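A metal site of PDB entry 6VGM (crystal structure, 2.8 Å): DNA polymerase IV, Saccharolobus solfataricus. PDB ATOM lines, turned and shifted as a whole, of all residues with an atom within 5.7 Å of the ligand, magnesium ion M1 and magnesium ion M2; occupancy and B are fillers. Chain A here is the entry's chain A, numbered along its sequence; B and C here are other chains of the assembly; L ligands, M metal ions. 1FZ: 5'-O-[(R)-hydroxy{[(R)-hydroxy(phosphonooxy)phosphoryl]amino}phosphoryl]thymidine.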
ATOM      1  N   ASP A   7      15.336   9.569  11.332  1.00  0.00           N
ATOM      2  CA  ASP A   7      16.407   9.366  10.375  1.00  0.00           C
ATOM      3  C   ASP A   7      15.820   8.716   9.135  1.00  0.00           C
ATOM      4  O   ASP A   7      15.175   7.668   9.227  1.00  0.00           O
ATOM      5  CB  ASP A   7      17.531   8.503  10.953  1.00  0.00           C
ATOM      6  CG  ASP A   7      18.591   8.147   9.911  1.00  0.00           C
ATOM      7  OD1 ASP A   7      18.372   7.191   9.150  1.00  0.00           O
ATOM      8  OD2 ASP A   7      19.624   8.847   9.850  1.00  0.00           O
ATOM      9  N   PHE A   8      16.043   9.339   7.984  1.00  0.00           N
ATOM     10  CA  PHE A   8      15.451   8.872   6.747  1.00  0.00           C
ATOM     11  C   PHE A   8      16.069   7.538   6.331  1.00  0.00           C
ATOM     12  O   PHE A   8      17.213   7.230   6.670  1.00  0.00           O
ATOM     13  CB  PHE A   8      15.637   9.896   5.624  1.00  0.00           C
ATOM     14  CG  PHE A   8      15.317  11.313   6.033  1.00  0.00           C
ATOM     15  CD1 PHE A   8      14.439  11.586   7.081  1.00  0.00           C
ATOM     16  CD2 PHE A   8      15.896  12.380   5.358  1.00  0.00           C
ATOM     17  CE1 PHE A   8      14.156  12.890   7.450  1.00  0.00           C
ATOM     18  CE2 PHE A   8      15.607  13.687   5.720  1.00  0.00           C
ATOM     19  CZ  PHE A   8      14.739  13.947   6.767  1.00  0.00           C
ATOM     20  N   ASP A   9      15.286   6.731   5.613  1.00  0.00           N
ATOM     21  CA  ASP A   9      15.720   5.405   5.203  1.00  0.00           C
ATOM     22  C   ASP A   9      16.402   5.460   3.846  1.00  0.00           C
ATOM     23  O   ASP A   9      15.847   6.042   2.900  1.00  0.00           O
ATOM     24  CB  ASP A   9      14.528   4.444   5.159  1.00  0.00           C
ATOM     25  CG  ASP A   9      13.674   4.528   6.406  1.00  0.00           C
ATOM     26  OD1 ASP A   9      14.148   4.101   7.486  1.00  0.00           O
ATOM     27  OD2 ASP A   9      12.526   5.011   6.312  1.00  0.00           O
ATOM     28  N   TYR A  10      17.581   4.849   3.746  1.00  0.00           N
ATOM     29  CA  TYR A  10      18.445   4.890   2.560  1.00  0.00           C
ATOM     30  C   TYR A  10      18.291   6.213   1.812  1.00  0.00           C
ATOM     31  O   TYR A  10      17.927   6.226   0.636  1.00  0.00           O
ATOM     32  CB  TYR A  10      18.182   3.674   1.653  1.00  0.00           C
ATOM     33  CG  TYR A  10      16.770   3.541   1.097  1.00  0.00           C
ATOM     34  CD1 TYR A  10      15.743   3.013   1.862  1.00  0.00           C
ATOM     35  CD2 TYR A  10      16.491   3.899  -0.218  1.00  0.00           C
ATOM     36  CE1 TYR A  10      14.465   2.883   1.346  1.00  0.00           C
ATOM     37  CE2 TYR A  10      15.223   3.776  -0.739  1.00  0.00           C
ATOM     38  CZ  TYR A  10      14.215   3.261   0.043  1.00  0.00           C
ATOM     39  OH  TYR A  10      12.951   3.127  -0.486  1.00  0.00           O
ATOM     40  N   PHE A  11      18.596   7.325   2.486  1.00  0.00           N
ATOM     41  CA  PHE A  11      18.078   8.630   2.076  1.00  0.00           C
ATOM     42  C   PHE A  11      18.394   8.962   0.623  1.00  0.00           C
ATOM     43  O   PHE A  11      17.491   9.262  -0.168  1.00  0.00           O
ATOM     44  CB  PHE A  11      18.636   9.725   2.999  1.00  0.00           C
ATOM     45  CG  PHE A  11      18.227  11.111   2.588  1.00  0.00           C
ATOM     46  CD1 PHE A  11      16.889  11.417   2.397  1.00  0.00           C
ATOM     47  CD2 PHE A  11      19.175  12.089   2.363  1.00  0.00           C
ATOM     48  CE1 PHE A  11      16.510  12.693   2.010  1.00  0.00           C
ATOM     49  CE2 PHE A  11      18.805  13.372   1.985  1.00  0.00           C
ATOM     50  CZ  PHE A  11      17.473  13.675   1.801  1.00  0.00           C
ATOM     51  N   TYR A  12      19.676   8.925   0.250  1.00  0.00           N
ATOM     52  CA  TYR A  12      20.071   9.370  -1.081  1.00  0.00           C
ATOM     53  C   TYR A  12      19.361   8.577  -2.171  1.00  0.00           C
ATOM     54  O   TYR A  12      18.874   9.153  -3.148  1.00  0.00           O
ATOM     55  CB  TYR A  12      21.590   9.243  -1.252  1.00  0.00           C
ATOM     56  CG  TYR A  12      22.392  10.343  -0.600  1.00  0.00           C
ATOM     57  CD1 TYR A  12      21.809  11.223   0.303  1.00  0.00           C
ATOM     58  CD2 TYR A  12      23.748  10.491  -0.885  1.00  0.00           C
ATOM     59  CE1 TYR A  12      22.556  12.221   0.900  1.00  0.00           C
ATOM     60  CE2 TYR A  12      24.498  11.477  -0.281  1.00  0.00           C
ATOM     61  CZ  TYR A  12      23.896  12.345   0.604  1.00  0.00           C
ATOM     62  OH  TYR A  12      24.641  13.334   1.200  1.00  0.00           O
ATOM     63  N   ALA A  13      19.279   7.256  -2.009  1.00  0.00           N
ATOM     64  CA  ALA A  13      18.654   6.413  -3.027  1.00  0.00           C
ATOM     65  C   ALA A  13      17.155   6.673  -3.131  1.00  0.00           C
ATOM     66  O   ALA A  13      16.612   6.743  -4.228  1.00  0.00           O
ATOM     67  CB  ALA A  13      18.925   4.940  -2.718  1.00  0.00           C
ATOM     68  N   VAL A  32      29.819   7.913  -5.391  1.00  0.00           N
ATOM     69  CA  VAL A  32      30.689   9.075  -5.470  1.00  0.00           C
ATOM     70  C   VAL A  32      31.858   8.668  -6.352  1.00  0.00           C
ATOM     71  O   VAL A  32      32.760   7.944  -5.911  1.00  0.00           O
ATOM     72  CB  VAL A  32      31.178   9.521  -4.087  1.00  0.00           C
ATOM     73  CG1 VAL A  32      31.752  10.938  -4.136  1.00  0.00           C
ATOM     74  CG2 VAL A  32      30.055   9.401  -3.063  1.00  0.00           C
ATOM     75  N   VAL A  43      30.697   3.939  -2.259  1.00  0.00           N
ATOM     76  CA  VAL A  43      29.239   3.872  -2.266  1.00  0.00           C
ATOM     77  C   VAL A  43      28.726   4.746  -1.136  1.00  0.00           C
ATOM     78  O   VAL A  43      29.046   4.514   0.035  1.00  0.00           O
ATOM     79  CB  VAL A  43      28.740   2.419  -2.144  1.00  0.00           C
ATOM     80  CG1 VAL A  43      27.247   2.398  -1.840  1.00  0.00           C
ATOM     81  CG2 VAL A  43      29.033   1.651  -3.415  1.00  0.00           C
ATOM     82  N   ALA A  44      27.937   5.768  -1.486  1.00  0.00           N
ATOM     83  CA  ALA A  44      27.325   6.620  -0.475  1.00  0.00           C
ATOM     84  C   ALA A  44      26.251   5.864   0.284  1.00  0.00           C
ATOM     85  O   ALA A  44      26.317   5.729   1.518  1.00  0.00           O
ATOM     86  CB  ALA A  44      26.765   7.883  -1.130  1.00  0.00           C
ATOM     87  N   THR A  45      25.247   5.375  -0.426  1.00  0.00           N
ATOM     88  CA  THR A  45      24.235   4.518   0.167  1.00  0.00           C
ATOM     89  C   THR A  45      23.643   3.631  -0.911  1.00  0.00           C
ATOM     90  O   THR A  45      23.783   3.894  -2.110  1.00  0.00           O
ATOM     91  CB  THR A  45      23.128   5.328   0.872  1.00  0.00           C
ATOM     92  OG1 THR A  45      22.538   4.537   1.911  1.00  0.00           O
ATOM     93  CG2 THR A  45      22.041   5.745  -0.128  1.00  0.00           C
ATOM     94  N   ALA A  46      23.003   2.549  -0.480  1.00  0.00           N
ATOM     95  CA  ALA A  46      22.262   1.669  -1.362  1.00  0.00           C
ATOM     96  C   ALA A  46      20.928   1.324  -0.700  1.00  0.00           C
ATOM     97  O   ALA A  46      20.841   1.220   0.524  1.00  0.00           O
ATOM     98  CB  ALA A  46      23.035   0.385  -1.678  1.00  0.00           C
ATOM     99  N   TYR A  48      17.574  -0.988   0.277  1.00  0.00           N
ATOM    100  CA  TYR A  48      17.601  -2.214   1.077  1.00  0.00           C
ATOM    101  C   TYR A  48      17.521  -3.480   0.230  1.00  0.00           C
ATOM    102  O   TYR A  48      17.955  -4.541   0.693  1.00  0.00           O
ATOM    103  CB  TYR A  48      16.486  -2.179   2.108  1.00  0.00           C
ATOM    104  CG  TYR A  48      16.874  -1.409   3.346  1.00  0.00           C
ATOM    105  CD1 TYR A  48      16.879  -0.013   3.337  1.00  0.00           C
ATOM    106  CD2 TYR A  48      17.277  -2.060   4.498  1.00  0.00           C
ATOM    107  CE1 TYR A  48      17.245   0.698   4.458  1.00  0.00           C
ATOM    108  CE2 TYR A  48      17.649  -1.352   5.626  1.00  0.00           C
ATOM    109  CZ  TYR A  48      17.635   0.032   5.600  1.00  0.00           C
ATOM    110  OH  TYR A  48      18.002   0.743   6.721  1.00  0.00           O
ATOM    111  N   ARG A  51      21.071  -3.456  -0.445  1.00  0.00           N
ATOM    112  CA  ARG A  51      21.741  -3.631   0.843  1.00  0.00           C
ATOM    113  C   ARG A  51      21.635  -5.071   1.331  1.00  0.00           C
ATOM    114  O   ARG A  51      22.501  -5.526   2.099  1.00  0.00           O
ATOM    115  CB  ARG A  51      21.159  -2.665   1.879  1.00  0.00           C
ATOM    116  CG  ARG A  51      22.083  -2.417   3.059  1.00  0.00           C
ATOM    117  CD  ARG A  51      21.516  -1.370   4.021  1.00  0.00           C
ATOM    118  NE  ARG A  51      21.202  -0.112   3.351  1.00  0.00           N
ATOM    119  CZ  ARG A  51      20.819   0.992   3.978  1.00  0.00           C
ATOM    120  NH1 ARG A  51      20.705   0.998   5.301  1.00  0.00           N
ATOM    121  NH2 ARG A  51      20.551   2.097   3.299  1.00  0.00           N
ATOM    122  N   ALA A  57      27.286   1.409   2.701  1.00  0.00           N
ATOM    123  CA  ALA A  57      28.043   2.659   2.645  1.00  0.00           C
ATOM    124  C   ALA A  57      29.519   2.398   2.933  1.00  0.00           C
ATOM    125  O   ALA A  57      29.869   1.605   3.818  1.00  0.00           O
ATOM    126  CB  ALA A  57      27.473   3.658   3.644  1.00  0.00           C
ATOM    127  N   GLY A  58      30.389   3.060   2.180  1.00  0.00           N
ATOM    128  CA  GLY A  58      31.817   2.999   2.389  1.00  0.00           C
ATOM    129  C   GLY A  58      32.558   1.977   1.568  1.00  0.00           C
ATOM    130  O   GLY A  58      33.796   1.969   1.574  1.00  0.00           O
ATOM    131  N   MET A  76      26.033  10.796  -7.382  1.00  0.00           N
ATOM    132  CA  MET A  76      25.357  11.534  -6.327  1.00  0.00           C
ATOM    133  C   MET A  76      25.004  12.942  -6.788  1.00  0.00           C
ATOM    134  O   MET A  76      25.834  13.637  -7.397  1.00  0.00           O
ATOM    135  CB  MET A  76      26.243  11.592  -5.075  1.00  0.00           C
ATOM    136  CG  MET A  76      25.486  11.853  -3.804  1.00  0.00           C
ATOM    137  SD  MET A  76      26.454  12.824  -2.632  1.00  0.00           S
ATOM    138  CE  MET A  76      28.091  12.196  -2.915  1.00  0.00           C
ATOM    139  N   SER A 103      22.292  15.816  10.916  1.00  0.00           N
ATOM    140  CA  SER A 103      22.985  15.585   9.657  1.00  0.00           C
ATOM    141  C   SER A 103      22.068  15.838   8.458  1.00  0.00           C
ATOM    142  O   SER A 103      21.039  16.501   8.591  1.00  0.00           O
ATOM    143  CB  SER A 103      23.524  14.149   9.579  1.00  0.00           C
ATOM    144  OG  SER A 103      22.522  13.202   9.918  1.00  0.00           O
ATOM    145  N   ILE A 104      22.453  15.310   7.298  1.00  0.00           N
ATOM    146  CA  ILE A 104      21.641  15.475   6.096  1.00  0.00           C
ATOM    147  C   ILE A 104      20.292  14.781   6.245  1.00  0.00           C
ATOM    148  O   ILE A 104      19.302  15.199   5.634  1.00  0.00           O
ATOM    149  CB  ILE A 104      22.408  14.961   4.857  1.00  0.00           C
ATOM    150  CG1 ILE A 104      21.686  15.335   3.562  1.00  0.00           C
ATOM    151  CG2 ILE A 104      22.594  13.450   4.917  1.00  0.00           C
ATOM    152  CD1 ILE A 104      21.583  16.826   3.327  1.00  0.00           C
ATOM    153  N   ASP A 105      20.212  13.726   7.072  1.00  0.00           N
ATOM    154  CA  ASP A 105      19.009  12.901   7.138  1.00  0.00           C
ATOM    155  C   ASP A 105      18.534  12.648   8.566  1.00  0.00           C
ATOM    156  O   ASP A 105      17.730  11.740   8.784  1.00  0.00           O
ATOM    157  CB  ASP A 105      19.238  11.568   6.402  1.00  0.00           C
ATOM    158  CG  ASP A 105      19.899  10.502   7.278  1.00  0.00           C
ATOM    159  OD1 ASP A 105      20.934  10.789   7.929  1.00  0.00           O
ATOM    160  OD2 ASP A 105      19.399   9.364   7.307  1.00  0.00           O
ATOM    161  N   GLU A 106      18.977  13.455   9.527  1.00  0.00           N
ATOM    162  CA  GLU A 106      18.705  13.159  10.932  1.00  0.00           C
ATOM    163  C   GLU A 106      18.252  14.405  11.680  1.00  0.00           C
ATOM    164  O   GLU A 106      18.755  15.503  11.439  1.00  0.00           O
ATOM    165  CB  GLU A 106      19.934  12.574  11.628  1.00  0.00           C
ATOM    166  CG  GLU A 106      20.254  11.173  11.185  1.00  0.00           C
ATOM    167  CD  GLU A 106      21.725  10.851  11.271  1.00  0.00           C
ATOM    168  OE1 GLU A 106      22.197  10.577  12.393  1.00  0.00           O
ATOM    169  OE2 GLU A 106      22.396  10.870  10.222  1.00  0.00           O
ATOM    170  N   LYS A 159      14.583   0.369  11.549  1.00  0.00           N
ATOM    171  CA  LYS A 159      14.748   0.609  10.113  1.00  0.00           C
ATOM    172  C   LYS A 159      14.458  -0.671   9.325  1.00  0.00           C
ATOM    173  O   LYS A 159      14.929  -1.743   9.711  1.00  0.00           O
ATOM    174  CB  LYS A 159      16.159   1.117   9.802  1.00  0.00           C
ATOM    175  CG  LYS A 159      16.646   2.203  10.725  1.00  0.00           C
ATOM    176  CD  LYS A 159      17.532   3.198   9.996  1.00  0.00           C
ATOM    177  CE  LYS A 159      16.716   4.095   9.091  1.00  0.00           C
ATOM    178  NZ  LYS A 159      16.457   5.463   9.607  1.00  0.00           N
ATOM    179  N   PRO A 160      13.730  -0.599   8.204  1.00  0.00           N
ATOM    180  CA  PRO A 160      13.171   0.630   7.616  1.00  0.00           C
ATOM    181  C   PRO A 160      11.682   0.831   7.863  1.00  0.00           C
ATOM    182  O   PRO A 160      11.044  -0.051   8.436  1.00  0.00           O
ATOM    183  CB  PRO A 160      13.436   0.431   6.124  1.00  0.00           C
ATOM    184  CG  PRO A 160      13.302  -1.062   5.936  1.00  0.00           C
ATOM    185  CD  PRO A 160      13.609  -1.731   7.271  1.00  0.00           C
ATOM    186  P   A38 B   5      38.665   7.105  -4.711  1.00  0.00           P
ATOM    187  O1P A38 B   5      38.735   6.322  -5.954  1.00  0.00           O
ATOM    188  O2P A38 B   5      39.912   7.435  -3.972  1.00  0.00           O
ATOM    189  O5' A38 B   5      37.244   7.615  -4.138  1.00  0.00           O
ATOM    190  C5' A38 B   5      37.245   8.790  -3.360  1.00  0.00           C
ATOM    191  C4' A38 B   5      35.915   9.492  -3.577  1.00  0.00           C
ATOM    192  O4' A38 B   5      34.780   8.680  -2.874  1.00  0.00           O
ATOM    193  C3' A38 B   5      35.924  10.665  -2.999  1.00  0.00           C
ATOM    194  O3' A38 B   5      35.050  11.565  -3.730  1.00  0.00           O
ATOM    195  C2' A38 B   5      35.309  10.429  -1.516  1.00  0.00           C
ATOM    196  C1' A38 B   5      34.312   9.602  -1.734  1.00  0.00           C
ATOM    197  N9  A38 B   5      34.032   8.796  -0.519  1.00  0.00           N
ATOM    198  C8  A38 B   5      34.905   7.859   0.114  1.00  0.00           C
ATOM    199  N7  A38 B   5      34.209   7.320   1.257  1.00  0.00           N
ATOM    200  C5  A38 B   5      32.878   7.965   1.333  1.00  0.00           C
ATOM    201  C6  A38 B   5      31.768   7.865   2.203  1.00  0.00           C
ATOM    202  N6  A38 B   5      31.814   6.975   3.329  1.00  0.00           N
ATOM    203  N1  A38 B   5      30.706   8.622   1.953  1.00  0.00           N
ATOM    204  C2  A38 B   5      30.625   9.465   0.919  1.00  0.00           C
ATOM    205  N3  A38 B   5      31.656   9.577   0.079  1.00  0.00           N
ATOM    206  C4  A38 B   5      32.771   8.856   0.260  1.00  0.00           C
ATOM    207  O   A38 B   5      35.986   7.567  -0.245  1.00  0.00           O
ATOM    208  P    DG B   6      36.017  12.743  -4.049  1.00  0.00           P
ATOM    209  OP1  DG B   6      35.477  13.167  -5.364  1.00  0.00           O
ATOM    210  OP2  DG B   6      37.475  12.799  -3.771  1.00  0.00           O
ATOM    211  O5'  DG B   6      35.246  13.541  -2.901  1.00  0.00           O
ATOM    212  C5'  DG B   6      33.838  13.702  -2.974  1.00  0.00           C
ATOM    213  C4'  DG B   6      33.248  14.045  -1.627  1.00  0.00           C
ATOM    214  O4'  DG B   6      33.326  12.915  -0.731  1.00  0.00           O
ATOM    215  C3'  DG B   6      33.923  15.201  -0.872  1.00  0.00           C
ATOM    216  O3'  DG B   6      33.031  16.318  -0.860  1.00  0.00           O
ATOM    217  C2'  DG B   6      34.160  14.647   0.558  1.00  0.00           C
ATOM    218  C1'  DG B   6      33.230  13.431   0.567  1.00  0.00           C
ATOM    219  N9   DG B   6      33.582  12.390   1.534  1.00  0.00           N
ATOM    220  C8   DG B   6      34.742  11.653   1.588  1.00  0.00           C
ATOM    221  N7   DG B   6      34.761  10.776   2.562  1.00  0.00           N
ATOM    222  C5   DG B   6      33.536  10.944   3.193  1.00  0.00           C
ATOM    223  C6   DG B   6      32.985  10.276   4.310  1.00  0.00           C
ATOM    224  O6   DG B   6      33.492   9.369   4.986  1.00  0.00           O
ATOM    225  N1   DG B   6      31.721  10.753   4.628  1.00  0.00           N
ATOM    226  C2   DG B   6      31.056  11.746   3.942  1.00  0.00           C
ATOM    227  N2   DG B   6      29.845  12.066   4.394  1.00  0.00           N
ATOM    228  N3   DG B   6      31.562  12.376   2.888  1.00  0.00           N
ATOM    229  C4   DG B   6      32.805  11.927   2.572  1.00  0.00           C
ATOM    230  P    DC C  13      25.585   7.570  12.199  1.00  0.00           P
ATOM    231  OP1  DC C  13      24.390   7.280  13.030  1.00  0.00           O
ATOM    232  OP2  DC C  13      26.349   6.465  11.583  1.00  0.00           O
ATOM    233  O5'  DC C  13      25.175   8.541  10.988  1.00  0.00           O
ATOM    234  C5'  DC C  13      25.150   9.963  11.152  1.00  0.00           C
ATOM    235  C4'  DC C  13      25.370  10.639   9.807  1.00  0.00           C
ATOM    236  O4'  DC C  13      26.780  10.582   9.429  1.00  0.00           O
ATOM    237  C3'  DC C  13      24.599  10.006   8.647  1.00  0.00           C
ATOM    238  O3'  DC C  13      24.008  11.025   7.842  1.00  0.00           O
ATOM    239  C2'  DC C  13      25.687   9.266   7.878  1.00  0.00           C
ATOM    240  C1'  DC C  13      26.846  10.213   8.069  1.00  0.00           C
ATOM    241  N1   DC C  13      28.172   9.587   7.758  1.00  0.00           N
ATOM    242  C2   DC C  13      28.980  10.149   6.765  1.00  0.00           C
ATOM    243  O2   DC C  13      28.597  11.170   6.186  1.00  0.00           O
ATOM    244  N3   DC C  13      30.178   9.571   6.485  1.00  0.00           N
ATOM    245  C4   DC C  13      30.556   8.477   7.133  1.00  0.00           C
ATOM    246  N4   DC C  13      31.741   7.942   6.814  1.00  0.00           N
ATOM    247  C5   DC C  13      29.743   7.882   8.143  1.00  0.00           C
ATOM    248  C6   DC C  13      28.566   8.454   8.416  1.00  0.00           C
HETATM  249  O2  1FZ L   1      27.579   9.569   2.013  1.00  0.00           O
HETATM  250  O4  1FZ L   1      29.360   6.522   4.866  1.00  0.00           O
HETATM  251  C4  1FZ L   1      28.382   7.184   4.503  1.00  0.00           C
HETATM  252  C5  1FZ L   1      27.167   7.100   5.152  1.00  0.00           C
HETATM  253  C6  1FZ L   1      26.109   7.867   4.695  1.00  0.00           C
HETATM  254  C5M 1FZ L   1      27.016   6.240   6.235  1.00  0.00           C
HETATM  255  N3  1FZ L   1      28.496   8.044   3.424  1.00  0.00           N
HETATM  256  C2  1FZ L   1      27.424   8.814   2.980  1.00  0.00           C
HETATM  257  N1  1FZ L   1      26.232   8.750   3.591  1.00  0.00           N
HETATM  258  C1' 1FZ L   1      25.114   9.615   3.049  1.00  0.00           C
HETATM  259  C2' 1FZ L   1      24.128   8.886   2.137  1.00  0.00           C
HETATM  260  C3' 1FZ L   1      23.198   8.283   3.172  1.00  0.00           C
HETATM  261  O3' 1FZ L   1      21.908   7.911   2.588  1.00  0.00           O
HETATM  262  O4' 1FZ L   1      24.181  10.281   3.958  1.00  0.00           O
HETATM  263  C4' 1FZ L   1      23.023   9.429   4.167  1.00  0.00           C
HETATM  264  C5' 1FZ L   1      23.210   8.904   5.581  1.00  0.00           C
HETATM  265  O5' 1FZ L   1      22.036   8.360   6.159  1.00  0.00           O
HETATM  266  PA  1FZ L   1      22.190   7.056   7.053  1.00  0.00           P
HETATM  267  O1A 1FZ L   1      21.267   7.016   8.220  1.00  0.00           O
HETATM  268  O2A 1FZ L   1      23.728   6.956   7.539  1.00  0.00           O
HETATM  269  N3A 1FZ L   1      22.079   5.787   6.024  1.00  0.00           N
HETATM  270  PB  1FZ L   1      20.767   5.851   5.030  1.00  0.00           P
HETATM  271  O1B 1FZ L   1      21.267   5.898   3.505  1.00  0.00           O
HETATM  272  O2B 1FZ L   1      19.722   6.879   5.311  1.00  0.00           O
HETATM  273  O3B 1FZ L   1      20.204   4.390   5.203  1.00  0.00           O
HETATM  274  PG  1FZ L   1      19.520   3.960   6.576  1.00  0.00           P
HETATM  275  O1G 1FZ L   1      19.386   5.246   7.543  1.00  0.00           O
HETATM  276  O3G 1FZ L   1      18.198   3.335   6.307  1.00  0.00           O
HETATM  277  O2G 1FZ L   1      20.560   2.979   7.339  1.00  0.00           O
HETATM  278 MG    MG M   1      19.166   7.317   7.124  1.00  0.00          MG
HETATM  279 MG    MG M   2      21.845   8.641   9.580  1.00  0.00          MG
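N3 of DC 13 of chain C lies close to N1 of DG 6 of chain B, at 2.7 Å. O of Asp 7 lies within hydrogen-bond range of NZ of Lys 159 (2.6 Å). The side-chain carboxylate of Glu 106 sits close to the side-chain carboxylate of Asp 105, at 2.7 Å. O3' of DC 13 of chain C is in hydrogen-bond range of the side-chain hydroxyl (OG) of Ser 103 (3.4 Å). The side-chain hydroxyl (OG1) of Thr 45 sits at hydrogen-bond distance from the guanidinium group (NH2) of Arg 51. The side-chain amino group (NZ) of Lys 159 lies within salt-bridge range of the side-chain carboxylate (OD1) of Asp 9 (3.4 Å). NH2 of Arg 51 lies within hydrogen-bond range of O of Ala 46. The side-chain hydroxyl of Tyr 48 sits at hydrogen-bond distance from the guanidinium group of Arg 51 (3.1 Å).
OG1 of Thr 45 lies within hydrogen-bond range of O1B of the ligand (2.5 Å). The backbone NH (N) of Tyr 12 is in hydrogen-bond range of an oxygen (O3') of the ligand (3.4 Å). N of Tyr 10 sits at hydrogen-bond distance from O3B of the ligand. O2G of the ligand is in salt-bridge range of NH1 of Arg 51 (2.8 Å). An oxygen (O1B) of the ligand lies within hydrogen-bond range of the backbone NH (N) of Phe 11 (3.2 Å). N1 of A38 5 of chain B sits at hydrogen-bond distance from a nitrogen (N3) of the ligand. O3G of the ligand sits at hydrogen-bond distance from OH of Tyr 48, at 2.6 Å. The side-chain amino group of Lys 159 lies close to an oxygen (O1G) of the ligand (3.6 Å).
DC 13 of chain C touches magnesium ion M2 (C3' to MG, 3.2 Å). Four residues have an atom within 4 Å of magnesium ion M2: Asp 7, Asp 105, Glu 106 and DC 13 of chain C. Along chain A the residues within 4 Å of magnesium ion M2 span positions 7 to 106. The nearest printed residue that does not touch magnesium ion M2 is Ser 103 (4.6 Å).
An oxygen (O4) of the ligand sits close to N4 of DC 13 of chain C. Merely in contact with the ligand: Asp 9 (3.4 Å), Ala 44 (3.6 Å), Ala 57 (3.6 Å) and Ile 104 (3.7 Å). Hydrophobic or aromatic side chains that line the ligand: Phe 11, Tyr 12, Ala 44, Tyr 48, Ala 57 and Ile 104. 16 residues have an atom within 4 Å of the ligand: Asp 7, Phe 8, Asp 9, Tyr 10, Phe 11, Tyr 12, Ala 44, Thr 45, Tyr 48, Arg 51, Ala 57, Ile 104, Asp 105, Lys 159, A38 5 of chain B and DC 13 of chain C. Along chain A the residues within 4 Å of the ligand span positions 7 to 159. The nearest printed residue that does not touch the ligand is DG 6 of chain B (4.1 Å).
O1A of the ligand binds magnesium ion M2, at 2.2 Å. OD2 of Asp 7 binds magnesium ion M2. Magnesium ion M2 is bound by OE2 of Glu 106 (2.4 Å). Magnesium ion M2 has three donor atoms within binding distance.
Magnesium ion M1 is bound by an oxygen (O2B) of the ligand, the backbone carbonyl oxygen of Phe 8, the side-chain carboxylate of Asp 105, an oxygen (O1G) of the ligand, the side-chain carboxylate of Asp 7 and an oxygen (O1A) of the ligand. Magnesium ion M1 has six donor atoms within binding distance.
Within 4 Å of magnesium ion M1: Asp 7, Phe 8 and Asp 105. The nearest printed residue that does not touch magnesium ion M1 is Lys 159 (4.1 Å).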
